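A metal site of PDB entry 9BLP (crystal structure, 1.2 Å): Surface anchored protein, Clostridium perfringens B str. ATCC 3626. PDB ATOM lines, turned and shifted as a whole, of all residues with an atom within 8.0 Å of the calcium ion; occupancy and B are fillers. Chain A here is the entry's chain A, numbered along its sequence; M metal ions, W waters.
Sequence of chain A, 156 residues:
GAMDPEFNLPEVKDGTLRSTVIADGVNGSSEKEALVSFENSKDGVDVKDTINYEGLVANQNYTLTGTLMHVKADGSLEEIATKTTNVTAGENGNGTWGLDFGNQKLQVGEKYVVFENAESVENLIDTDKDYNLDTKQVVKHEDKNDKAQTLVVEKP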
ATOM      1  N   ALA A  23       9.176  18.922  22.590  1.00  0.00           N
ATOM      2  CA  ALA A  23       8.636  17.673  23.170  1.00  0.00           C
ATOM      3  C   ALA A  23       9.748  16.626  23.136  1.00  0.00           C
ATOM      4  O   ALA A  23      10.146  16.237  22.027  1.00  0.00           O
ATOM      5  CB  ALA A  23       7.417  17.226  22.409  1.00  0.00           C
ATOM      6  N   ASP A  24      10.273  16.246  24.297  1.00  0.00           N
ATOM      7  CA  ASP A  24      11.462  15.357  24.367  1.00  0.00           C
ATOM      8  C   ASP A  24      12.558  15.900  23.449  1.00  0.00           C
ATOM      9  O   ASP A  24      13.256  15.124  22.769  1.00  0.00           O
ATOM     10  CB  ASP A  24      11.070  13.914  24.011  1.00  0.00           C
ATOM     11  CG  ASP A  24      10.577  13.098  25.194  1.00  0.00           C
ATOM     12  OD1 ASP A  24      10.768  13.524  26.355  1.00  0.00           O
ATOM     13  OD2 ASP A  24      10.028  12.013  24.944  1.00  0.00           O
ATOM     14  N   GLY A  25      12.738  17.224  23.429  1.00  0.00           N
ATOM     15  CA  GLY A  25      13.819  17.875  22.675  1.00  0.00           C
ATOM     16  C   GLY A  25      13.526  18.028  21.201  1.00  0.00           C
ATOM     17  O   GLY A  25      14.423  18.506  20.485  1.00  0.00           O
ATOM     18  N   VAL A  36       7.206  12.708  18.267  1.00  0.00           N
ATOM     19  CA  VAL A  36       7.848  12.069  19.443  1.00  0.00           C
ATOM     20  C   VAL A  36       7.821  10.559  19.224  1.00  0.00           C
ATOM     21  O   VAL A  36       6.727   9.976  19.201  1.00  0.00           O
ATOM     22  CB  VAL A  36       7.142  12.470  20.746  1.00  0.00           C
ATOM     23  CG1 VAL A  36       7.790  11.806  21.942  1.00  0.00           C
ATOM     24  CG2 VAL A  36       7.103  13.983  20.925  1.00  0.00           C
ATOM     25  N   SER A  37       8.981   9.942  19.072  1.00  0.00           N
ATOM     26  CA  SER A  37       9.065   8.484  18.859  1.00  0.00           C
ATOM     27  C   SER A  37       8.456   7.781  20.076  1.00  0.00           C
ATOM     28  O   SER A  37       8.524   8.302  21.203  1.00  0.00           O
ATOM     29  CB  SER A  37      10.482   8.052  18.642  1.00  0.00           C
ATOM     30  OG  SER A  37      11.219   8.185  19.836  1.00  0.00           O
ATOM     31  N   PHE A  38       7.886   6.604  19.855  1.00  0.00           N
ATOM     32  CA  PHE A  38       7.341   5.803  20.974  1.00  0.00           C
ATOM     33  C   PHE A  38       8.435   5.592  22.015  1.00  0.00           C
ATOM     34  O   PHE A  38       8.167   5.721  23.235  1.00  0.00           O
ATOM     35  CB  PHE A  38       6.819   4.437  20.524  1.00  0.00           C
ATOM     36  CG  PHE A  38       6.366   3.657  21.731  1.00  0.00           C
ATOM     37  CD1 PHE A  38       5.227   4.041  22.398  1.00  0.00           C
ATOM     38  CD2 PHE A  38       7.152   2.655  22.281  1.00  0.00           C
ATOM     39  CE1 PHE A  38       4.814   3.395  23.554  1.00  0.00           C
ATOM     40  CE2 PHE A  38       6.747   2.015  23.437  1.00  0.00           C
ATOM     41  CZ  PHE A  38       5.582   2.377  24.065  1.00  0.00           C
ATOM     42  N   GLU A  39       9.661   5.296  21.572  1.00  0.00           N
ATOM     43  CA  GLU A  39      10.811   5.030  22.479  1.00  0.00           C
ATOM     44  C   GLU A  39      11.009   6.250  23.387  1.00  0.00           C
ATOM     45  O   GLU A  39      11.080   6.050  24.617  1.00  0.00           O
ATOM     46  CB  GLU A  39      12.088   4.729  21.694  1.00  0.00           C
ATOM     47  CG  GLU A  39      13.185   4.107  22.534  1.00  0.00           C
ATOM     48  CD  GLU A  39      12.892   2.723  23.060  1.00  0.00           C
ATOM     49  OE1 GLU A  39      13.173   2.469  24.247  1.00  0.00           O
ATOM     50  OE2 GLU A  39      12.384   1.884  22.287  1.00  0.00           O
ATOM     51  N   ASN A  40      11.059   7.445  22.802  1.00  0.00           N
ATOM     52  CA  ASN A  40      11.219   8.718  23.560  1.00  0.00           C
ATOM     53  C   ASN A  40      10.096   8.815  24.590  1.00  0.00           C
ATOM     54  O   ASN A  40      10.370   9.201  25.732  1.00  0.00           O
ATOM     55  CB  ASN A  40      11.245   9.957  22.650  1.00  0.00           C
ATOM     56  CG  ASN A  40      12.618  10.232  22.086  1.00  0.00           C
ATOM     57  OD1 ASN A  40      13.588   9.585  22.453  1.00  0.00           O
ATOM     58  ND2 ASN A  40      12.695  11.184  21.172  1.00  0.00           N
ATOM     59  N   SER A  41       8.877   8.446  24.206  1.00  0.00           N
ATOM     60  CA  SER A  41       7.662   8.622  25.050  1.00  0.00           C
ATOM     61  C   SER A  41       7.637   7.649  26.232  1.00  0.00           C
ATOM     62  O   SER A  41       6.843   7.883  27.146  1.00  0.00           O
ATOM     63  CB  SER A  41       6.405   8.469  24.229  1.00  0.00           C
ATOM     64  OG  SER A  41       6.058   7.097  24.066  1.00  0.00           O
ATOM     65  N   LYS A  42       8.455   6.585  26.234  1.00  0.00           N
ATOM     66  CA  LYS A  42       8.353   5.501  27.243  1.00  0.00           C
ATOM     67  C   LYS A  42       8.602   6.042  28.648  1.00  0.00           C
ATOM     68  O   LYS A  42       8.062   5.471  29.606  1.00  0.00           O
ATOM     69  CB  LYS A  42       9.363   4.376  27.000  1.00  0.00           C
ATOM     70  CG  LYS A  42       9.025   3.418  25.873  1.00  0.00           C
ATOM     71  CD  LYS A  42      10.114   2.385  25.693  1.00  0.00           C
ATOM     72  CE  LYS A  42       9.708   1.221  24.829  1.00  0.00           C
ATOM     73  NZ  LYS A  42      10.749   0.173  24.787  1.00  0.00           N
ATOM     74  N   ASP A  43       9.452   7.066  28.782  1.00  0.00           N
ATOM     75  CA  ASP A  43       9.748   7.670  30.109  1.00  0.00           C
ATOM     76  C   ASP A  43       8.970   8.976  30.253  1.00  0.00           C
ATOM     77  O   ASP A  43       9.438   9.871  30.981  1.00  0.00           O
ATOM     78  CB  ASP A  43      11.259   7.816  30.335  1.00  0.00           C
ATOM     79  CG  ASP A  43      11.989   8.743  29.375  1.00  0.00           C
ATOM     80  OD1 ASP A  43      11.383   9.182  28.365  1.00  0.00           O
ATOM     81  OD2 ASP A  43      13.165   9.013  29.649  1.00  0.00           O
ATOM     82  N   GLY A  44       7.817   9.081  29.612  1.00  0.00           N
ATOM     83  CA  GLY A  44       7.051  10.336  29.551  1.00  0.00           C
ATOM     84  C   GLY A  44       7.654  11.264  28.523  1.00  0.00           C
ATOM     85  O   GLY A  44       8.731  10.955  27.952  1.00  0.00           O
ATOM     86  N   VAL A  45       7.000  12.391  28.307  1.00  0.00           N
ATOM     87  CA  VAL A  45       7.430  13.390  27.299  1.00  0.00           C
ATOM     88  C   VAL A  45       7.696  14.682  28.053  1.00  0.00           C
ATOM     89  O   VAL A  45       6.768  15.214  28.672  1.00  0.00           O
ATOM     90  CB  VAL A  45       6.387  13.565  26.181  1.00  0.00           C
ATOM     91  CG1 VAL A  45       6.851  14.582  25.160  1.00  0.00           C
ATOM     92  CG2 VAL A  45       6.042  12.242  25.513  1.00  0.00           C
ATOM     93  N   ASP A  46       8.929  15.169  28.017  1.00  0.00           N
ATOM     94  CA  ASP A  46       9.263  16.491  28.577  1.00  0.00           C
ATOM     95  C   ASP A  46       8.677  17.550  27.648  1.00  0.00           C
ATOM     96  O   ASP A  46       9.002  17.525  26.463  1.00  0.00           O
ATOM     97  CB  ASP A  46      10.782  16.629  28.711  1.00  0.00           C
ATOM     98  CG  ASP A  46      11.364  15.553  29.603  1.00  0.00           C
ATOM     99  OD1 ASP A  46      10.804  15.352  30.689  1.00  0.00           O
ATOM    100  OD2 ASP A  46      12.310  14.872  29.152  1.00  0.00           O
ATOM    101  N   ASN A 103       7.535  16.699  32.800  1.00  0.00           N
ATOM    102  CA  ASN A 103       7.354  15.387  32.169  1.00  0.00           C
ATOM    103  C   ASN A 103       5.860  15.045  32.180  1.00  0.00           C
ATOM    104  O   ASN A 103       5.249  15.074  33.257  1.00  0.00           O
ATOM    105  CB  ASN A 103       8.239  14.367  32.885  1.00  0.00           C
ATOM    106  CG  ASN A 103       8.297  13.037  32.159  1.00  0.00           C
ATOM    107  OD1 ASN A 103       9.201  12.796  31.355  1.00  0.00           O
ATOM    108  ND2 ASN A 103       7.332  12.187  32.452  1.00  0.00           N
ATOM    109  N   GLN A 104       5.299  14.768  31.001  1.00  0.00           N
ATOM    110  CA  GLN A 104       3.859  14.500  30.823  1.00  0.00           C
ATOM    111  C   GLN A 104       3.685  13.078  30.283  1.00  0.00           C
ATOM    112  O   GLN A 104       4.468  12.646  29.433  1.00  0.00           O
ATOM    113  CB  GLN A 104       3.254  15.528  29.881  1.00  0.00           C
ATOM    114  CG  GLN A 104       3.343  16.953  30.411  1.00  0.00           C
ATOM    115  CD  GLN A 104       2.495  17.230  31.645  1.00  0.00           C
ATOM    116  OE1 GLN A 104       2.863  18.022  32.503  1.00  0.00           O
ATOM    117  NE2 GLN A 104       1.372  16.559  31.733  1.00  0.00           N
ATOM    118  N   LYS A 105       2.671  12.374  30.766  1.00  0.00           N
ATOM    119  CA  LYS A 105       2.448  10.959  30.387  1.00  0.00           C
ATOM    120  C   LYS A 105       1.545  10.952  29.154  1.00  0.00           C
ATOM    121  O   LYS A 105       0.345  10.689  29.277  1.00  0.00           O
ATOM    122  CB  LYS A 105       1.928  10.171  31.589  1.00  0.00           C
ATOM    123  CG  LYS A 105       2.841  10.218  32.810  1.00  0.00           C
ATOM    124  CD  LYS A 105       4.300   9.879  32.535  1.00  0.00           C
ATOM    125  CE  LYS A 105       5.183   9.975  33.768  1.00  0.00           C
ATOM    126  NZ  LYS A 105       6.564   9.498  33.499  1.00  0.00           N
HETATM  127 CA    CA M   1      10.854  11.064  27.050  1.00  0.00          CA
HETATM  128  O   HOH W   1      13.019  11.116  26.098  1.00  0.00           O
HETATM  129  O   HOH W   2      11.638  12.181  29.012  1.00  0.00           O
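Four residues have an atom within 4 Å of the calcium ion: Asp 24, Asn 40, Asp 43 and Gly 44.
The nearest printed residue that does not touch the calcium ion is Val 45 (4.1 Å).
Water W2 lies within hydrogen-bond range of OD2 of Asp 46 and OD1 of Asn 103.
The calcium ion is bound by O of Gly 44.
The calcium ion is bound by the backbone carbonyl oxygen (O) of Asn 40, 2.3 Å away.
The side-chain carboxylate (OD1) of Asp 43 is bound to the calcium ion, 2.4 Å away.
The calcium ion is bound by water W1 (2.4 Å).
The calcium ion is bound by water W2 (2.4 Å).
The calcium ion is bound by the side-chain carboxylate (OD2) of Asp 24 (2.5 Å).
OD1 of Asp 24 binds the calcium ion (2.6 Å).
The calcium ion has seven donor atoms within binding distance.
The side-chain amide oxygen of Asn 103 lies close to the backbone carbonyl oxygen of Asp 43, at 3.0 Å.
OG of Ser 37 is in hydrogen-bond range of N of Asn 40 (3.1 Å).
The backbone carbonyl oxygen (O) of Asp 46 is in hydrogen-bond range of the backbone NH (N) of Asp 24.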
